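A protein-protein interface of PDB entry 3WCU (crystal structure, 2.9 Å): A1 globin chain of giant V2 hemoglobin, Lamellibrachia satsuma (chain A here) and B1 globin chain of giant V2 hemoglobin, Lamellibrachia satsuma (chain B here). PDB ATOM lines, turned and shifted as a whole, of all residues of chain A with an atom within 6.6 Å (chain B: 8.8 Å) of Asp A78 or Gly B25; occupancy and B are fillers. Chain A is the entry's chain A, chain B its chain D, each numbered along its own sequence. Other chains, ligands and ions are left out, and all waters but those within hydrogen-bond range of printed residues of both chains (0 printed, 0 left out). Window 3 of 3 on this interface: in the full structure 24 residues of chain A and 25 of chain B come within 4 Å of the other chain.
Of the 14 printed residues of chain B, 7 touch a printed residue of chain A.
Printed residues of chain B that touch a printed residue of chain A: Ala B22, Ile B24, Gly B25, Ala B26, Arg B29, Trp B30 and His B65.
Among the printed residues, 10 pairs touch across the chains.
Among the printed residues, no Asp or Glu carboxylate lies within 4 Å of a Lys or Arg side-chain nitrogen of the other chain.
Of the printed residues of chain B, Asp A78 touches Gly B25 and Ala B26.
Of the printed residues of chain B, Asn A79 touches Ala B26 (3.9 Å), Trp B30 (3.9 Å) and His B65 (3.6 Å).
Of the printed residues of chain A, Gly B25 touches Lys A11 and Asp A78.
Printed residues of chain A within 4 Å of Ala B26: Asp A78 (2.7 Å) and Asn A79 (3.9 Å).
The nearest residue of chain A that does not touch Gly B25 is Ser A75 (5.8 Å).
O of Ile B24 is in hydrogen-bond range of NZ of Lys A11, at 2.7 Å.
The backbone NH (N) of Ala B26 lies within hydrogen-bond range of the side-chain carboxylate (OD2) of Asp A78 (2.7 Å).
The side-chain amino group (NZ) of Lys A11 lies within hydrogen-bond range of the backbone carbonyl oxygen (O) of Ser A75, at 3.5 Å.
The side-chain amino group of Lys A11 is in salt-bridge range of the side-chain carboxylate of Asp A78 (3.6 Å).
The backbone carbonyl oxygen (O) of Asn B21 is in hydrogen-bond range of the guanidinium group (NH1) of Arg B29, at 3.4 Å.
O of Ile B24 is in hydrogen-bond range of NH1 of Arg B29 (2.9 Å).
A ring nitrogen (NE2) of His B65 is in hydrogen-bond range of the backbone NH of Trp B30, at 3.3 Å.
CE of Lys A11 touches O of Ala B22, 2.8 Å away.
Gly B25 touches Lys A11 (CA to NZ, 3.96 Å).
OG of Ser A75 touches CB of Ala B22, at 3.1 Å.
Ser A75 touches Arg B29.
C of Gly B25 touches OD2 of Asp A78, 3.7 Å away.
Asn A79 touches Ala B26 (CB to CB, 3.9 Å).
ND2 of Asn A79 touches CE3 of Trp B30, at 3.9 Å.
Asn A79 touches His B65.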
ATOM      1  N   ILE A   4     -23.918  24.139 -29.073  1.00  0.00           N
ATOM      2  CA  ILE A   4     -23.408  24.906 -27.932  1.00  0.00           C
ATOM      3  C   ILE A   4     -23.212  26.429 -28.155  1.00  0.00           C
ATOM      4  O   ILE A   4     -23.431  27.221 -27.233  1.00  0.00           O
ATOM      5  CB  ILE A   4     -22.081  24.305 -27.441  1.00  0.00           C
ATOM      6  CG1 ILE A   4     -21.300  25.340 -26.611  1.00  0.00           C
ATOM      7  CG2 ILE A   4     -21.298  23.782 -28.634  1.00  0.00           C
ATOM      8  CD1 ILE A   4     -21.775  25.467 -25.143  1.00  0.00           C
ATOM      9  N   ARG A   7     -26.296  28.043 -27.513  1.00  0.00           N
ATOM     10  CA  ARG A   7     -26.656  27.840 -26.118  1.00  0.00           C
ATOM     11  C   ARG A   7     -25.946  28.908 -25.277  1.00  0.00           C
ATOM     12  O   ARG A   7     -26.579  29.584 -24.465  1.00  0.00           O
ATOM     13  CB  ARG A   7     -26.282  26.417 -25.677  1.00  0.00           C
ATOM     14  CG  ARG A   7     -27.195  25.355 -26.279  1.00  0.00           C
ATOM     15  CD  ARG A   7     -26.691  23.925 -26.080  1.00  0.00           C
ATOM     16  NE  ARG A   7     -27.666  22.955 -26.582  1.00  0.00           N
ATOM     17  CZ  ARG A   7     -28.223  22.007 -25.837  1.00  0.00           C
ATOM     18  NH1 ARG A   7     -27.894  21.901 -24.561  1.00  0.00           N
ATOM     19  NH2 ARG A   7     -29.127  21.182 -26.352  1.00  0.00           N
ATOM     20  N   LEU A   8     -24.642  29.077 -25.485  1.00  0.00           N
ATOM     21  CA  LEU A   8     -23.892  30.100 -24.760  1.00  0.00           C
ATOM     22  C   LEU A   8     -24.476  31.484 -25.058  1.00  0.00           C
ATOM     23  O   LEU A   8     -24.410  32.386 -24.217  1.00  0.00           O
ATOM     24  CB  LEU A   8     -22.411  30.081 -25.156  1.00  0.00           C
ATOM     25  CG  LEU A   8     -21.598  28.891 -24.638  1.00  0.00           C
ATOM     26  CD1 LEU A   8     -20.117  29.078 -24.931  1.00  0.00           C
ATOM     27  CD2 LEU A   8     -21.791  28.778 -23.149  1.00  0.00           C
ATOM     28  N   LYS A  11     -27.920  32.083 -23.449  1.00  0.00           N
ATOM     29  CA  LYS A  11     -27.686  32.316 -22.032  1.00  0.00           C
ATOM     30  C   LYS A  11     -27.403  33.800 -21.789  1.00  0.00           C
ATOM     31  O   LYS A  11     -27.988  34.409 -20.889  1.00  0.00           O
ATOM     32  CB  LYS A  11     -26.513  31.468 -21.509  1.00  0.00           C
ATOM     33  CG  LYS A  11     -26.809  29.977 -21.370  1.00  0.00           C
ATOM     34  CD  LYS A  11     -25.634  29.222 -20.761  1.00  0.00           C
ATOM     35  CE  LYS A  11     -25.497  29.532 -19.278  1.00  0.00           C
ATOM     36  NZ  LYS A  11     -24.218  29.060 -18.674  1.00  0.00           N
ATOM     37  N   VAL A  73     -33.180  26.317 -15.951  1.00  0.00           N
ATOM     38  CA  VAL A  73     -33.069  25.440 -17.104  1.00  0.00           C
ATOM     39  C   VAL A  73     -32.063  26.049 -18.096  1.00  0.00           C
ATOM     40  O   VAL A  73     -30.991  25.476 -18.318  1.00  0.00           O
ATOM     41  CB  VAL A  73     -34.441  25.231 -17.769  1.00  0.00           C
ATOM     42  CG1 VAL A  73     -34.300  24.390 -19.034  1.00  0.00           C
ATOM     43  CG2 VAL A  73     -35.368  24.538 -16.791  1.00  0.00           C
ATOM     44  N   ILE A  74     -32.389  27.213 -18.664  1.00  0.00           N
ATOM     45  CA  ILE A  74     -31.489  27.892 -19.608  1.00  0.00           C
ATOM     46  C   ILE A  74     -30.055  27.998 -19.078  1.00  0.00           C
ATOM     47  O   ILE A  74     -29.100  27.953 -19.844  1.00  0.00           O
ATOM     48  CB  ILE A  74     -31.990  29.335 -19.953  1.00  0.00           C
ATOM     49  CG1 ILE A  74     -33.324  29.259 -20.700  1.00  0.00           C
ATOM     50  CG2 ILE A  74     -30.950  30.093 -20.818  1.00  0.00           C
ATOM     51  CD1 ILE A  74     -33.916  30.623 -21.006  1.00  0.00           C
ATOM     52  N   SER A  75     -29.905  28.138 -17.768  1.00  0.00           N
ATOM     53  CA  SER A  75     -28.588  28.262 -17.174  1.00  0.00           C
ATOM     54  C   SER A  75     -27.773  26.990 -17.327  1.00  0.00           C
ATOM     55  O   SER A  75     -26.553  27.014 -17.164  1.00  0.00           O
ATOM     56  CB  SER A  75     -28.701  28.616 -15.690  1.00  0.00           C
ATOM     57  OG  SER A  75     -29.211  29.926 -15.502  1.00  0.00           O
ATOM     58  N   MET A  76     -28.433  25.879 -17.638  1.00  0.00           N
ATOM     59  CA  MET A  76     -27.717  24.614 -17.790  1.00  0.00           C
ATOM     60  C   MET A  76     -27.546  24.172 -19.246  1.00  0.00           C
ATOM     61  O   MET A  76     -26.954  23.132 -19.517  1.00  0.00           O
ATOM     62  CB  MET A  76     -28.407  23.512 -16.972  1.00  0.00           C
ATOM     63  CG  MET A  76     -28.488  23.821 -15.477  1.00  0.00           C
ATOM     64  SD  MET A  76     -28.892  22.433 -14.364  1.00  0.00           S
ATOM     65  CE  MET A  76     -30.690  22.440 -14.390  1.00  0.00           C
ATOM     66  N   PHE A  77     -28.056  24.968 -20.179  1.00  0.00           N
ATOM     67  CA  PHE A  77     -27.955  24.668 -21.605  1.00  0.00           C
ATOM     68  C   PHE A  77     -26.575  24.140 -21.996  1.00  0.00           C
ATOM     69  O   PHE A  77     -26.421  23.513 -23.038  1.00  0.00           O
ATOM     70  CB  PHE A  77     -28.216  25.928 -22.428  1.00  0.00           C
ATOM     71  CG  PHE A  77     -29.628  26.077 -22.931  1.00  0.00           C
ATOM     72  CD1 PHE A  77     -30.151  25.203 -23.865  1.00  0.00           C
ATOM     73  CD2 PHE A  77     -30.400  27.157 -22.540  1.00  0.00           C
ATOM     74  CE1 PHE A  77     -31.427  25.416 -24.406  1.00  0.00           C
ATOM     75  CE2 PHE A  77     -31.667  27.372 -23.074  1.00  0.00           C
ATOM     76  CZ  PHE A  77     -32.179  26.505 -24.006  1.00  0.00           C
ATOM     77  N   ASP A  78     -25.561  24.400 -21.183  1.00  0.00           N
ATOM     78  CA  ASP A  78     -24.223  23.947 -21.535  1.00  0.00           C
ATOM     79  C   ASP A  78     -23.756  22.682 -20.800  1.00  0.00           C
ATOM     80  O   ASP A  78     -22.555  22.384 -20.754  1.00  0.00           O
ATOM     81  CB  ASP A  78     -23.223  25.089 -21.317  1.00  0.00           C
ATOM     82  CG  ASP A  78     -23.182  25.565 -19.880  1.00  0.00           C
ATOM     83  OD1 ASP A  78     -24.234  25.529 -19.207  1.00  0.00           O
ATOM     84  OD2 ASP A  78     -22.096  25.988 -19.428  1.00  0.00           O
ATOM     85  N   ASN A  79     -24.713  21.948 -20.231  1.00  0.00           N
ATOM     86  CA  ASN A  79     -24.435  20.706 -19.509  1.00  0.00           C
ATOM     87  C   ASN A  79     -25.586  19.721 -19.735  1.00  0.00           C
ATOM     88  O   ASN A  79     -26.488  19.594 -18.901  1.00  0.00           O
ATOM     89  CB  ASN A  79     -24.264  20.983 -18.011  1.00  0.00           C
ATOM     90  CG  ASN A  79     -24.027  19.717 -17.197  1.00  0.00           C
ATOM     91  OD1 ASN A  79     -24.775  18.747 -17.303  1.00  0.00           O
ATOM     92  ND2 ASN A  79     -22.986  19.729 -16.366  1.00  0.00           N
ATOM     93  N   GLU A  80     -25.541  19.050 -20.887  1.00  0.00           N
ATOM     94  CA  GLU A  80     -26.524  18.047 -21.300  1.00  0.00           C
ATOM     95  C   GLU A  80     -27.035  17.183 -20.151  1.00  0.00           C
ATOM     96  O   GLU A  80     -28.237  16.990 -19.997  1.00  0.00           O
ATOM     97  CB  GLU A  80     -25.903  17.124 -22.350  1.00  0.00           C
ATOM     98  CG  GLU A  80     -25.806  17.701 -23.738  1.00  0.00           C
ATOM     99  CD  GLU A  80     -27.133  17.661 -24.448  1.00  0.00           C
ATOM    100  OE1 GLU A  80     -27.746  16.572 -24.486  1.00  0.00           O
ATOM    101  OE2 GLU A  80     -27.564  18.711 -24.969  1.00  0.00           O
ATOM    102  N   LEU A  83     -28.749  19.450 -17.451  1.00  0.00           N
ATOM    103  CA  LEU A  83     -29.909  19.952 -18.185  1.00  0.00           C
ATOM    104  C   LEU A  83     -30.983  18.886 -18.374  1.00  0.00           C
ATOM    105  O   LEU A  83     -32.174  19.135 -18.157  1.00  0.00           O
ATOM    106  CB  LEU A  83     -29.516  20.495 -19.572  1.00  0.00           C
ATOM    107  CG  LEU A  83     -30.698  20.721 -20.542  1.00  0.00           C
ATOM    108  CD1 LEU A  83     -31.710  21.650 -19.934  1.00  0.00           C
ATOM    109  CD2 LEU A  83     -30.218  21.303 -21.843  1.00  0.00           C
ATOM    110  N   ILE B  19     -22.005  36.619  -8.531  1.00  0.00           N
ATOM    111  CA  ILE B  19     -21.569  35.240  -8.648  1.00  0.00           C
ATOM    112  C   ILE B  19     -22.663  34.248  -9.019  1.00  0.00           C
ATOM    113  O   ILE B  19     -22.435  33.043  -9.033  1.00  0.00           O
ATOM    114  CB  ILE B  19     -20.922  34.776  -7.342  1.00  0.00           C
ATOM    115  CG1 ILE B  19     -21.956  34.848  -6.218  1.00  0.00           C
ATOM    116  CG2 ILE B  19     -19.702  35.634  -7.037  1.00  0.00           C
ATOM    117  CD1 ILE B  19     -21.468  34.312  -4.902  1.00  0.00           C
ATOM    118  N   ASN B  21     -25.819  33.892 -11.904  1.00  0.00           N
ATOM    119  CA  ASN B  21     -26.707  34.337 -12.970  1.00  0.00           C
ATOM    120  C   ASN B  21     -26.549  33.399 -14.151  1.00  0.00           C
ATOM    121  O   ASN B  21     -25.552  32.685 -14.256  1.00  0.00           O
ATOM    122  CB  ASN B  21     -26.422  35.790 -13.372  1.00  0.00           C
ATOM    123  CG  ASN B  21     -25.012  36.000 -13.884  1.00  0.00           C
ATOM    124  OD1 ASN B  21     -24.692  35.683 -15.031  1.00  0.00           O
ATOM    125  ND2 ASN B  21     -24.156  36.541 -13.028  1.00  0.00           N
ATOM    126  N   ALA B  22     -27.546  33.394 -15.025  1.00  0.00           N
ATOM    127  CA  ALA B  22     -27.550  32.517 -16.182  1.00  0.00           C
ATOM    128  C   ALA B  22     -26.413  32.717 -17.170  1.00  0.00           C
ATOM    129  O   ALA B  22     -26.291  31.985 -18.151  1.00  0.00           O
ATOM    130  CB  ALA B  22     -28.847  32.656 -16.896  1.00  0.00           C
ATOM    131  N   GLY B  23     -25.580  33.711 -16.933  1.00  0.00           N
ATOM    132  CA  GLY B  23     -24.498  33.939 -17.863  1.00  0.00           C
ATOM    133  C   GLY B  23     -23.255  33.184 -17.467  1.00  0.00           C
ATOM    134  O   GLY B  23     -22.273  33.191 -18.205  1.00  0.00           O
ATOM    135  N   ILE B  24     -23.310  32.517 -16.317  1.00  0.00           N
ATOM    136  CA  ILE B  24     -22.169  31.772 -15.793  1.00  0.00           C
ATOM    137  C   ILE B  24     -22.039  30.337 -16.307  1.00  0.00           C
ATOM    138  O   ILE B  24     -23.009  29.574 -16.322  1.00  0.00           O
ATOM    139  CB  ILE B  24     -22.183  31.815 -14.244  1.00  0.00           C
ATOM    140  CG1 ILE B  24     -22.102  33.278 -13.800  1.00  0.00           C
ATOM    141  CG2 ILE B  24     -21.008  31.055 -13.670  1.00  0.00           C
ATOM    142  CD1 ILE B  24     -21.919  33.477 -12.326  1.00  0.00           C
ATOM    143  N   GLY B  25     -20.823  30.006 -16.752  1.00  0.00           N
ATOM    144  CA  GLY B  25     -20.524  28.693 -17.299  1.00  0.00           C
ATOM    145  C   GLY B  25     -20.850  27.557 -16.355  1.00  0.00           C
ATOM    146  O   GLY B  25     -20.437  27.578 -15.197  1.00  0.00           O
ATOM    147  N   ALA B  26     -21.583  26.564 -16.861  1.00  0.00           N
ATOM    148  CA  ALA B  26     -21.997  25.392 -16.085  1.00  0.00           C
ATOM    149  C   ALA B  26     -20.880  24.846 -15.203  1.00  0.00           C
ATOM    150  O   ALA B  26     -21.138  24.157 -14.216  1.00  0.00           O
ATOM    151  CB  ALA B  26     -22.496  24.298 -17.023  1.00  0.00           C
ATOM    152  N   LYS B  27     -19.644  25.166 -15.571  1.00  0.00           N
ATOM    153  CA  LYS B  27     -18.462  24.724 -14.841  1.00  0.00           C
ATOM    154  C   LYS B  27     -18.372  25.323 -13.441  1.00  0.00           C
ATOM    155  O   LYS B  27     -17.878  24.689 -12.511  1.00  0.00           O
ATOM    156  CB  LYS B  27     -17.201  25.072 -15.639  1.00  0.00           C
ATOM    157  CG  LYS B  27     -15.955  24.338 -15.177  1.00  0.00           C
ATOM    158  CD  LYS B  27     -16.239  22.848 -14.992  1.00  0.00           C
ATOM    159  CE  LYS B  27     -16.862  22.230 -16.243  1.00  0.00           C
ATOM    160  NZ  LYS B  27     -17.475  20.890 -15.978  1.00  0.00           N
ATOM    161  N   SER B  28     -18.841  26.555 -13.289  1.00  0.00           N
ATOM    162  CA  SER B  28     -18.810  27.191 -11.987  1.00  0.00           C
ATOM    163  C   SER B  28     -19.997  26.751 -11.153  1.00  0.00           C
ATOM    164  O   SER B  28     -19.844  26.490  -9.962  1.00  0.00           O
ATOM    165  CB  SER B  28     -18.817  28.709 -12.131  1.00  0.00           C
ATOM    166  OG  SER B  28     -17.551  29.172 -12.548  1.00  0.00           O
ATOM    167  N   ARG B  29     -21.174  26.666 -11.774  1.00  0.00           N
ATOM    168  CA  ARG B  29     -22.373  26.253 -11.054  1.00  0.00           C
ATOM    169  C   ARG B  29     -22.030  24.988 -10.295  1.00  0.00           C
ATOM    170  O   ARG B  29     -22.199  24.910  -9.077  1.00  0.00           O
ATOM    171  CB  ARG B  29     -23.518  25.942 -12.001  1.00  0.00           C
ATOM    172  CG  ARG B  29     -23.448  26.656 -13.297  1.00  0.00           C
ATOM    173  CD  ARG B  29     -24.784  26.584 -13.982  1.00  0.00           C
ATOM    174  NE  ARG B  29     -25.744  27.426 -13.285  1.00  0.00           N
ATOM    175  CZ  ARG B  29     -25.703  28.753 -13.293  1.00  0.00           C
ATOM    176  NH1 ARG B  29     -24.754  29.383 -13.968  1.00  0.00           N
ATOM    177  NH2 ARG B  29     -26.604  29.452 -12.616  1.00  0.00           N
ATOM    178  N   TRP B  30     -21.537  24.004 -11.035  1.00  0.00           N
ATOM    179  CA  TRP B  30     -21.144  22.722 -10.471  1.00  0.00           C
ATOM    180  C   TRP B  30     -20.230  22.908  -9.262  1.00  0.00           C
ATOM    181  O   TRP B  30     -20.477  22.361  -8.184  1.00  0.00           O
ATOM    182  CB  TRP B  30     -20.414  21.909 -11.534  1.00  0.00           C
ATOM    183  CG  TRP B  30     -20.078  20.515 -11.131  1.00  0.00           C
ATOM    184  CD1 TRP B  30     -19.450  20.110  -9.985  1.00  0.00           C
ATOM    185  CD2 TRP B  30     -20.299  19.336 -11.905  1.00  0.00           C
ATOM    186  NE1 TRP B  30     -19.265  18.752 -10.001  1.00  0.00           N
ATOM    187  CE2 TRP B  30     -19.776  18.251 -11.170  1.00  0.00           C
ATOM    188  CE3 TRP B  30     -20.888  19.090 -13.156  1.00  0.00           C
ATOM    189  CZ2 TRP B  30     -19.823  16.935 -11.645  1.00  0.00           C
ATOM    190  CZ3 TRP B  30     -20.935  17.781 -13.629  1.00  0.00           C
ATOM    191  CH2 TRP B  30     -20.405  16.720 -12.873  1.00  0.00           C
ATOM    192  N   THR B  31     -19.166  23.680  -9.451  1.00  0.00           N
ATOM    193  CA  THR B  31     -18.212  23.911  -8.381  1.00  0.00           C
ATOM    194  C   THR B  31     -18.897  24.472  -7.135  1.00  0.00           C
ATOM    195  O   THR B  31     -18.514  24.148  -6.008  1.00  0.00           O
ATOM    196  CB  THR B  31     -17.086  24.857  -8.849  1.00  0.00           C
ATOM    197  OG1 THR B  31     -16.508  24.342 -10.055  1.00  0.00           O
ATOM    198  CG2 THR B  31     -15.998  24.971  -7.788  1.00  0.00           C
ATOM    199  N   MET B  32     -19.922  25.297  -7.328  1.00  0.00           N
ATOM    200  CA  MET B  32     -20.647  25.869  -6.195  1.00  0.00           C
ATOM    201  C   MET B  32     -21.555  24.836  -5.537  1.00  0.00           C
ATOM    202  O   MET B  32     -21.591  24.717  -4.309  1.00  0.00           O
ATOM    203  CB  MET B  32     -21.466  27.077  -6.643  1.00  0.00           C
ATOM    204  CG  MET B  32     -20.627  28.313  -6.882  1.00  0.00           C
ATOM    205  SD  MET B  32     -21.617  29.671  -7.473  1.00  0.00           S
ATOM    206  CE  MET B  32     -22.667  29.978  -6.052  1.00  0.00           C
ATOM    207  N   HIS B  65     -26.351  17.265  -9.873  1.00  0.00           N
ATOM    208  CA  HIS B  65     -26.045  18.644 -10.210  1.00  0.00           C
ATOM    209  C   HIS B  65     -27.347  19.409 -10.372  1.00  0.00           C
ATOM    210  O   HIS B  65     -27.513  20.483  -9.796  1.00  0.00           O
ATOM    211  CB  HIS B  65     -25.242  18.737 -11.505  1.00  0.00           C
ATOM    212  CG  HIS B  65     -24.766  20.124 -11.810  1.00  0.00           C
ATOM    213  ND1 HIS B  65     -24.292  20.495 -13.050  1.00  0.00           N
ATOM    214  CD2 HIS B  65     -24.685  21.228 -11.030  1.00  0.00           C
ATOM    215  CE1 HIS B  65     -23.939  21.769 -13.020  1.00  0.00           C
ATOM    216  NE2 HIS B  65     -24.168  22.236 -11.806  1.00  0.00           N
